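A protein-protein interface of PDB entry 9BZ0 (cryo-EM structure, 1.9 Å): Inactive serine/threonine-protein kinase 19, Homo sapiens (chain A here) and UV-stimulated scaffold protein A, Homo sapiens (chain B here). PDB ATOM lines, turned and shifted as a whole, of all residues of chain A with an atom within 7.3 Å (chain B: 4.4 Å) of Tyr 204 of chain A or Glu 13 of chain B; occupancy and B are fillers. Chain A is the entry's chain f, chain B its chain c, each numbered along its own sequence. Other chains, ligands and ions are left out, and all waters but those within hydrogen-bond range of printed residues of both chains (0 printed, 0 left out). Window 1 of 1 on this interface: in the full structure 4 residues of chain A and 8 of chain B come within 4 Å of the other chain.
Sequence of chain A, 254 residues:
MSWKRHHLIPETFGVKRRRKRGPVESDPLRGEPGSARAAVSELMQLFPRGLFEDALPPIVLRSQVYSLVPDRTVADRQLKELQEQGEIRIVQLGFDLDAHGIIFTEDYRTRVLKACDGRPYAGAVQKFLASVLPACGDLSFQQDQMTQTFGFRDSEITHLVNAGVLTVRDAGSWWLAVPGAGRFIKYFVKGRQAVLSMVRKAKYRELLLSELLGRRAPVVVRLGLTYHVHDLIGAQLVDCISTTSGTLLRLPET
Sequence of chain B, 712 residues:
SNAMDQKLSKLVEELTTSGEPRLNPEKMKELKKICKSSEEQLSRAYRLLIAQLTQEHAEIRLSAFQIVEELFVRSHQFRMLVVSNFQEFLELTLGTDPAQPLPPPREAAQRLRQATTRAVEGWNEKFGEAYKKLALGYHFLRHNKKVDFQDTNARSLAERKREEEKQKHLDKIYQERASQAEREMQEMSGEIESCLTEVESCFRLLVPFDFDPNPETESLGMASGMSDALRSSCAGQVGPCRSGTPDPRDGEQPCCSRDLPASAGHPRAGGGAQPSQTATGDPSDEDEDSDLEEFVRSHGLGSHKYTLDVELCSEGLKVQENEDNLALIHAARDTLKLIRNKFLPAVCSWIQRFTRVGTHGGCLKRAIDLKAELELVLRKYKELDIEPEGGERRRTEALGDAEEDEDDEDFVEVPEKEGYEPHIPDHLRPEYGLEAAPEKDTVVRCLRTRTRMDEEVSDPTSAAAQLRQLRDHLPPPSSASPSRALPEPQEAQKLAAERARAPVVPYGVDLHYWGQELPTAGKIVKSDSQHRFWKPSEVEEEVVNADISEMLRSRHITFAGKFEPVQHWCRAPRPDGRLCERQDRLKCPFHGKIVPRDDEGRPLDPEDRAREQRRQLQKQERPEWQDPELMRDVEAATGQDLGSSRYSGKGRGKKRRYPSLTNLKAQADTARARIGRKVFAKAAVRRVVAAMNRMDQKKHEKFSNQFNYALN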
ATOM      1  N   VAL A 199       7.856  14.811  -8.769  1.00  0.00           N
ATOM      2  CA  VAL A 199       8.014  14.371 -10.152  1.00  0.00           C
ATOM      3  C   VAL A 199       6.785  13.633 -10.645  1.00  0.00           C
ATOM      4  O   VAL A 199       6.337  13.837 -11.777  1.00  0.00           O
ATOM      5  CB  VAL A 199       9.281  13.518 -10.302  1.00  0.00           C
ATOM      6  CG1 VAL A 199       9.450  13.101 -11.735  1.00  0.00           C
ATOM      7  CG2 VAL A 199      10.487  14.296  -9.840  1.00  0.00           C
ATOM      8  N   ARG A 200       6.219  12.769  -9.813  1.00  0.00           N
ATOM      9  CA  ARG A 200       5.052  11.992 -10.219  1.00  0.00           C
ATOM     10  C   ARG A 200       3.840  12.861 -10.535  1.00  0.00           C
ATOM     11  O   ARG A 200       3.067  12.546 -11.443  1.00  0.00           O
ATOM     12  CB  ARG A 200       4.715  10.989  -9.123  1.00  0.00           C
ATOM     13  CG  ARG A 200       3.721   9.928  -9.519  1.00  0.00           C
ATOM     14  CD  ARG A 200       3.230   9.186  -8.296  1.00  0.00           C
ATOM     15  NE  ARG A 200       4.313   8.474  -7.631  1.00  0.00           N
ATOM     16  CZ  ARG A 200       4.255   8.011  -6.389  1.00  0.00           C
ATOM     17  NH1 ARG A 200       5.301   7.357  -5.890  1.00  0.00           N
ATOM     18  NH2 ARG A 200       3.185   8.192  -5.633  1.00  0.00           N
ATOM     19  N   LYS A 201       3.648  13.940  -9.799  1.00  0.00           N
ATOM     20  CA  LYS A 201       2.484  14.790  -9.971  1.00  0.00           C
ATOM     21  C   LYS A 201       2.658  15.854 -11.036  1.00  0.00           C
ATOM     22  O   LYS A 201       1.659  16.317 -11.597  1.00  0.00           O
ATOM     23  CB  LYS A 201       2.118  15.458  -8.647  1.00  0.00           C
ATOM     24  CG  LYS A 201       1.560  14.503  -7.617  1.00  0.00           C
ATOM     25  CD  LYS A 201       1.186  15.236  -6.341  1.00  0.00           C
ATOM     26  CE  LYS A 201       0.630  14.281  -5.299  1.00  0.00           C
ATOM     27  NZ  LYS A 201       0.233  14.990  -4.051  1.00  0.00           N
ATOM     28  N   ALA A 202       3.885  16.261 -11.329  1.00  0.00           N
ATOM     29  CA  ALA A 202       4.080  17.258 -12.360  1.00  0.00           C
ATOM     30  C   ALA A 202       3.614  16.738 -13.716  1.00  0.00           C
ATOM     31  O   ALA A 202       3.456  15.535 -13.938  1.00  0.00           O
ATOM     32  CB  ALA A 202       5.547  17.668 -12.427  1.00  0.00           C
ATOM     33  N   LYS A 203       3.365  17.684 -14.616  1.00  0.00           N
ATOM     34  CA  LYS A 203       2.905  17.397 -15.968  1.00  0.00           C
ATOM     35  C   LYS A 203       3.824  16.398 -16.667  1.00  0.00           C
ATOM     36  O   LYS A 203       5.049  16.469 -16.551  1.00  0.00           O
ATOM     37  CB  LYS A 203       2.797  18.719 -16.724  1.00  0.00           C
ATOM     38  CG  LYS A 203       1.727  18.776 -17.792  1.00  0.00           C
ATOM     39  CD  LYS A 203       1.813  20.098 -18.539  1.00  0.00           C
ATOM     40  CE  LYS A 203       2.708  20.049 -19.746  1.00  0.00           C
ATOM     41  NZ  LYS A 203       1.877  19.858 -20.962  1.00  0.00           N
ATOM     42  N   TYR A 204       3.217  15.466 -17.394  1.00  0.00           N
ATOM     43  CA  TYR A 204       3.854  14.325 -18.050  1.00  0.00           C
ATOM     44  C   TYR A 204       4.646  13.418 -17.119  1.00  0.00           C
ATOM     45  O   TYR A 204       5.373  12.546 -17.607  1.00  0.00           O
ATOM     46  CB  TYR A 204       4.794  14.731 -19.190  1.00  0.00           C
ATOM     47  CG  TYR A 204       4.305  15.772 -20.149  1.00  0.00           C
ATOM     48  CD1 TYR A 204       3.032  15.703 -20.690  1.00  0.00           C
ATOM     49  CD2 TYR A 204       5.152  16.779 -20.582  1.00  0.00           C
ATOM     50  CE1 TYR A 204       2.591  16.652 -21.576  1.00  0.00           C
ATOM     51  CE2 TYR A 204       4.729  17.719 -21.482  1.00  0.00           C
ATOM     52  CZ  TYR A 204       3.451  17.649 -21.978  1.00  0.00           C
ATOM     53  OH  TYR A 204       3.033  18.586 -22.886  1.00  0.00           O
ATOM     54  N   ARG A 205       4.558  13.599 -15.803  1.00  0.00           N
ATOM     55  CA  ARG A 205       5.525  13.034 -14.863  1.00  0.00           C
ATOM     56  C   ARG A 205       6.945  13.506 -15.146  1.00  0.00           C
ATOM     57  O   ARG A 205       7.910  12.862 -14.731  1.00  0.00           O
ATOM     58  CB  ARG A 205       5.510  11.496 -14.860  1.00  0.00           C
ATOM     59  CG  ARG A 205       4.192  10.795 -15.176  1.00  0.00           C
ATOM     60  CD  ARG A 205       3.112  11.086 -14.173  1.00  0.00           C
ATOM     61  NE  ARG A 205       1.902  10.328 -14.461  1.00  0.00           N
ATOM     62  CZ  ARG A 205       0.881  10.199 -13.626  1.00  0.00           C
ATOM     63  NH1 ARG A 205      -0.159   9.451 -13.981  1.00  0.00           N
ATOM     64  NH2 ARG A 205       0.866  10.813 -12.454  1.00  0.00           N
ATOM     65  N   GLU A 206       7.099  14.611 -15.858  1.00  0.00           N
ATOM     66  CA  GLU A 206       8.398  15.178 -16.171  1.00  0.00           C
ATOM     67  C   GLU A 206       8.617  16.384 -15.282  1.00  0.00           C
ATOM     68  O   GLU A 206       7.678  17.137 -15.010  1.00  0.00           O
ATOM     69  CB  GLU A 206       8.460  15.591 -17.639  1.00  0.00           C
ATOM     70  CG  GLU A 206       8.816  14.464 -18.580  1.00  0.00           C
ATOM     71  CD  GLU A 206       9.057  14.947 -19.993  1.00  0.00           C
ATOM     72  OE1 GLU A 206       8.929  16.165 -20.235  1.00  0.00           O
ATOM     73  OE2 GLU A 206       9.379  14.109 -20.860  1.00  0.00           O
ATOM     74  N   LEU A 207       9.848  16.577 -14.826  1.00  0.00           N
ATOM     75  CA  LEU A 207      10.190  17.867 -14.254  1.00  0.00           C
ATOM     76  C   LEU A 207      11.642  18.203 -14.546  1.00  0.00           C
ATOM     77  O   LEU A 207      12.522  17.362 -14.359  1.00  0.00           O
ATOM     78  CB  LEU A 207       9.917  17.866 -12.751  1.00  0.00           C
ATOM     79  CG  LEU A 207       9.988  19.212 -12.041  1.00  0.00           C
ATOM     80  CD1 LEU A 207       9.038  20.196 -12.697  1.00  0.00           C
ATOM     81  CD2 LEU A 207       9.628  19.032 -10.585  1.00  0.00           C
ATOM     82  N   LEU A 249      14.013  15.119 -15.133  1.00  0.00           N
ATOM     83  CA  LEU A 249      13.711  13.966 -14.307  1.00  0.00           C
ATOM     84  C   LEU A 249      12.504  13.233 -14.863  1.00  0.00           C
ATOM     85  O   LEU A 249      11.543  13.851 -15.323  1.00  0.00           O
ATOM     86  CB  LEU A 249      13.431  14.395 -12.877  1.00  0.00           C
ATOM     87  CG  LEU A 249      14.511  15.192 -12.186  1.00  0.00           C
ATOM     88  CD1 LEU A 249      14.021  15.601 -10.843  1.00  0.00           C
ATOM     89  CD2 LEU A 249      15.751  14.355 -12.060  1.00  0.00           C
ATOM     90  N   ARG A 250      12.560  11.909 -14.823  1.00  0.00           N
ATOM     91  CA  ARG A 250      11.431  11.098 -15.226  1.00  0.00           C
ATOM     92  C   ARG A 250      11.251   9.938 -14.267  1.00  0.00           C
ATOM     93  O   ARG A 250      12.200   9.482 -13.629  1.00  0.00           O
ATOM     94  CB  ARG A 250      11.623  10.552 -16.636  1.00  0.00           C
ATOM     95  CG  ARG A 250      11.500  11.589 -17.728  1.00  0.00           C
ATOM     96  CD  ARG A 250      11.623  10.930 -19.086  1.00  0.00           C
ATOM     97  NE  ARG A 250      10.462  10.100 -19.377  1.00  0.00           N
ATOM     98  CZ  ARG A 250      10.502   8.784 -19.535  1.00  0.00           C
ATOM     99  NH1 ARG A 250       9.381   8.130 -19.819  1.00  0.00           N
ATOM    100  NH2 ARG A 250      11.631   8.108 -19.402  1.00  0.00           N
ATOM    101  N   LEU A 251      10.020   9.471 -14.180  1.00  0.00           N
ATOM    102  CA  LEU A 251       9.744   8.167 -13.604  1.00  0.00           C
ATOM    103  C   LEU A 251      10.169   7.079 -14.579  1.00  0.00           C
ATOM    104  O   LEU A 251       9.851   7.163 -15.769  1.00  0.00           O
ATOM    105  CB  LEU A 251       8.265   8.046 -13.288  1.00  0.00           C
ATOM    106  CG  LEU A 251       7.744   9.109 -12.325  1.00  0.00           C
ATOM    107  CD1 LEU A 251       6.270   8.888 -12.027  1.00  0.00           C
ATOM    108  CD2 LEU A 251       8.562   9.117 -11.045  1.00  0.00           C
ATOM    109  N   SER B   9       3.602  21.282 -25.995  1.00  0.00           N
ATOM    110  CA  SER B   9       2.960  21.108 -24.697  1.00  0.00           C
ATOM    111  C   SER B   9       1.518  21.601 -24.698  1.00  0.00           C
ATOM    112  O   SER B   9       0.600  20.888 -24.268  1.00  0.00           O
ATOM    113  CB  SER B   9       3.765  21.837 -23.623  1.00  0.00           C
ATOM    114  OG  SER B   9       3.134  21.739 -22.362  1.00  0.00           O
ATOM    115  N   LYS B  10       1.293  22.804 -25.215  1.00  0.00           N
ATOM    116  CA  LYS B  10      -0.057  23.350 -25.218  1.00  0.00           C
ATOM    117  C   LYS B  10      -0.966  22.588 -26.166  1.00  0.00           C
ATOM    118  O   LYS B  10      -2.133  22.347 -25.847  1.00  0.00           O
ATOM    119  CB  LYS B  10      -0.013  24.835 -25.578  1.00  0.00           C
ATOM    120  CG  LYS B  10       0.583  25.708 -24.483  1.00  0.00           C
ATOM    121  CD  LYS B  10       0.653  27.168 -24.893  1.00  0.00           C
ATOM    122  CE  LYS B  10       1.221  28.023 -23.770  1.00  0.00           C
ATOM    123  NZ  LYS B  10       1.240  29.470 -24.121  1.00  0.00           N
ATOM    124  N   LEU B  11      -0.466  22.213 -27.336  1.00  0.00           N
ATOM    125  CA  LEU B  11      -1.277  21.430 -28.257  1.00  0.00           C
ATOM    126  C   LEU B  11      -1.706  20.104 -27.640  1.00  0.00           C
ATOM    127  O   LEU B  11      -2.876  19.723 -27.728  1.00  0.00           O
ATOM    128  CB  LEU B  11      -0.524  21.208 -29.565  1.00  0.00           C
ATOM    129  CG  LEU B  11      -0.472  22.454 -30.452  1.00  0.00           C
ATOM    130  CD1 LEU B  11       0.550  22.290 -31.555  1.00  0.00           C
ATOM    131  CD2 LEU B  11      -1.845  22.755 -31.034  1.00  0.00           C
ATOM    132  N   VAL B  12      -0.772  19.372 -27.034  1.00  0.00           N
ATOM    133  CA  VAL B  12      -1.136  18.074 -26.466  1.00  0.00           C
ATOM    134  C   VAL B  12      -2.032  18.212 -25.239  1.00  0.00           C
ATOM    135  O   VAL B  12      -2.907  17.367 -25.015  1.00  0.00           O
ATOM    136  CB  VAL B  12       0.116  17.238 -26.142  1.00  0.00           C
ATOM    137  CG1 VAL B  12       0.919  16.970 -27.407  1.00  0.00           C
ATOM    138  CG2 VAL B  12       0.958  17.909 -25.086  1.00  0.00           C
ATOM    139  N   GLU B  13      -1.904  19.295 -24.468  1.00  0.00           N
ATOM    140  CA  GLU B  13      -2.896  19.544 -23.425  1.00  0.00           C
ATOM    141  C   GLU B  13      -4.270  19.804 -24.022  1.00  0.00           C
ATOM    142  O   GLU B  13      -5.249  19.137 -23.671  1.00  0.00           O
ATOM    143  CB  GLU B  13      -2.468  20.720 -22.549  1.00  0.00           C
ATOM    144  CG  GLU B  13      -1.239  20.457 -21.705  1.00  0.00           C
ATOM    145  CD  GLU B  13      -1.322  19.148 -20.947  1.00  0.00           C
ATOM    146  OE1 GLU B  13      -2.354  18.909 -20.287  1.00  0.00           O
ATOM    147  OE2 GLU B  13      -0.356  18.358 -21.014  1.00  0.00           O
ATOM    148  N   GLU B  14      -4.365  20.776 -24.920  1.00  0.00           N
ATOM    149  CA  GLU B  14      -5.666  21.174 -25.436  1.00  0.00           C
ATOM    150  C   GLU B  14      -6.324  20.044 -26.216  1.00  0.00           C
ATOM    151  O   GLU B  14      -7.555  19.967 -26.278  1.00  0.00           O
ATOM    152  CB  GLU B  14      -5.511  22.431 -26.290  1.00  0.00           C
ATOM    153  CG  GLU B  14      -5.172  23.665 -25.457  1.00  0.00           C
ATOM    154  CD  GLU B  14      -4.973  24.915 -26.289  1.00  0.00           C
ATOM    155  OE1 GLU B  14      -5.455  24.955 -27.437  1.00  0.00           O
ATOM    156  OE2 GLU B  14      -4.327  25.861 -25.790  1.00  0.00           O
ATOM    157  N   LEU B  15      -5.525  19.157 -26.808  1.00  0.00           N
ATOM    158  CA  LEU B  15      -6.076  17.950 -27.405  1.00  0.00           C
ATOM    159  C   LEU B  15      -6.522  16.940 -26.355  1.00  0.00           C
ATOM    160  O   LEU B  15      -7.534  16.258 -26.549  1.00  0.00           O
ATOM    161  CB  LEU B  15      -5.053  17.333 -28.347  1.00  0.00           C
ATOM    162  CG  LEU B  15      -4.898  18.112 -29.650  1.00  0.00           C
ATOM    163  CD1 LEU B  15      -3.666  17.657 -30.408  1.00  0.00           C
ATOM    164  CD2 LEU B  15      -6.144  17.942 -30.496  1.00  0.00           C
ATOM    165  N   THR B  16      -5.794  16.811 -25.243  1.00  0.00           N
ATOM    166  CA  THR B  16      -6.104  15.709 -24.338  1.00  0.00           C
ATOM    167  C   THR B  16      -6.938  16.113 -23.132  1.00  0.00           C
ATOM    168  O   THR B  16      -7.619  15.253 -22.565  1.00  0.00           O
ATOM    169  CB  THR B  16      -4.827  15.025 -23.838  1.00  0.00           C
ATOM    170  OG1 THR B  16      -4.052  15.946 -23.058  1.00  0.00           O
ATOM    171  CG2 THR B  16      -4.008  14.490 -25.006  1.00  0.00           C
ATOM    172  N   THR B  17      -6.912  17.373 -22.716  1.00  0.00           N
ATOM    173  CA  THR B  17      -7.921  17.825 -21.765  1.00  0.00           C
ATOM    174  C   THR B  17      -9.261  18.129 -22.420  1.00  0.00           C
ATOM    175  O   THR B  17     -10.202  18.496 -21.710  1.00  0.00           O
ATOM    176  CB  THR B  17      -7.442  19.071 -21.015  1.00  0.00           C
ATOM    177  OG1 THR B  17      -7.354  20.174 -21.924  1.00  0.00           O
ATOM    178  CG2 THR B  17      -6.086  18.828 -20.374  1.00  0.00           C
ATOM    179  N   SER B  18      -9.368  18.005 -23.746  1.00  0.00           N
ATOM    180  CA  SER B  18     -10.567  18.474 -24.434  1.00  0.00           C
ATOM    181  C   SER B  18     -11.812  17.698 -24.027  1.00  0.00           C
ATOM    182  O   SER B  18     -12.902  18.274 -23.949  1.00  0.00           O
ATOM    183  CB  SER B  18     -10.367  18.387 -25.945  1.00  0.00           C
ATOM    184  OG  SER B  18     -10.258  17.038 -26.364  1.00  0.00           O
ATOM    185  N   LEU B  48       5.414  12.440 -24.435  1.00  0.00           N
ATOM    186  CA  LEU B  48       4.261  13.098 -23.826  1.00  0.00           C
ATOM    187  C   LEU B  48       3.020  12.218 -23.852  1.00  0.00           C
ATOM    188  O   LEU B  48       2.347  12.049 -22.830  1.00  0.00           O
ATOM    189  CB  LEU B  48       3.972  14.411 -24.524  1.00  0.00           C
ATOM    190  CG  LEU B  48       4.810  15.525 -23.905  1.00  0.00           C
ATOM    191  CD1 LEU B  48       6.290  15.192 -24.057  1.00  0.00           C
ATOM    192  CD2 LEU B  48       4.509  16.840 -24.615  1.00  0.00           C
ATOM    193  N   ALA B  51       2.964   9.218 -21.495  1.00  0.00           N
ATOM    194  CA  ALA B  51       2.675   9.707 -20.152  1.00  0.00           C
ATOM    195  C   ALA B  51       1.209  10.094 -20.007  1.00  0.00           C
ATOM    196  O   ALA B  51       0.578   9.803 -18.986  1.00  0.00           O
ATOM    197  CB  ALA B  51       3.576  10.896 -19.820  1.00  0.00           C
ATOM    198  N   GLN B  52       0.657  10.769 -21.012  1.00  0.00           N
ATOM    199  CA  GLN B  52      -0.750  11.150 -20.974  1.00  0.00           C
ATOM    200  C   GLN B  52      -1.675   9.941 -20.974  1.00  0.00           C
ATOM    201  O   GLN B  52      -2.749   9.985 -20.366  1.00  0.00           O
ATOM    202  CB  GLN B  52      -1.051  12.060 -22.160  1.00  0.00           C
ATOM    203  CG  GLN B  52      -2.270  12.918 -22.000  1.00  0.00           C
ATOM    204  CD  GLN B  52      -2.026  14.114 -21.109  1.00  0.00           C
ATOM    205  OE1 GLN B  52      -2.317  14.082 -19.915  1.00  0.00           O
ATOM    206  NE2 GLN B  52      -1.495  15.183 -21.686  1.00  0.00           N
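The side-chain carboxylate (OE2) of Glu 13 of chain B sits at hydrogen-bond distance from the side-chain amide nitrogen (NE2) of Gln 52 of chain B (3.4 Å). The backbone carbonyl oxygen of Glu 13 of chain B lies within hydrogen-bond range of the side-chain hydroxyl of Thr 17 of chain B. The side-chain amino group (NZ) of Lys 203 of chain A sits at hydrogen-bond distance from the side-chain hydroxyl (OH) of Tyr 204 of chain A, at 2.6 Å. The side-chain hydroxyl (OG1) of Thr 16 of chain B is in hydrogen-bond range of the backbone carbonyl oxygen (O) of Val 12 of chain B (2.7 Å). OG1 of Thr 16 of chain B is in hydrogen-bond range of O of Glu 13 of chain B (3.5 Å).
Among the printed residues, pairs that only touch across the chains: Tyr 204 of chain A with Val 12 of chain B (3.1 Å), Tyr 204 of chain A with Glu 13 of chain B (3.5 Å), Tyr 204 of chain A with Leu 48 of chain B (2.9 Å) and Tyr 204 of chain A with Ala 51 of chain B (3.3 Å).
OG of Ser 9 of chain B sits close to OH of Tyr 204 of chain A (3.2 Å). OE2 of Glu 13 of chain B lies within salt-bridge range of NZ of Lys 203 of chain A, at 2.7 Å. The side-chain hydroxyl of Ser 9 of chain B lies within hydrogen-bond range of the side-chain amino group of Lys 203 of chain A.
Of the 13 printed residues of chain B, 5 touch a printed residue of chain A. Hydrophobic or aromatic side chains of chain A within 4 Å of the printed part of chain B: Tyr 204. Along chain A the printed residues that touch a printed residue of chain B span positions 203 to 204. Among the printed residues, 7 pairs touch across the chains. Among the printed residues, Asp or Glu carboxylates within 4 Å of a Lys or Arg side-chain nitrogen of the other chain: Lys 203 of chain A with Glu 13 of chain B.
Of the printed residues of chain B, Tyr 204 of chain A touches Ser 9, Val 12, Glu 13, Leu 48 and Ala 51. Glu 13 of chain B touches two residues of chain A. Of the printed residues of chain A, Ser 9 of chain B touches Lys 203 (2.7 Å) and Tyr 204 (3.1 Å). Printed residues of chain A within 4 Å of Ala 51 of chain B: Tyr 204. Gln 52 of chain B touches none of the printed residues of chain A. The nearest printed residue of chain A that does not touch Glu 13 of chain B is Ala 202 of chain A (8.5 Å).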
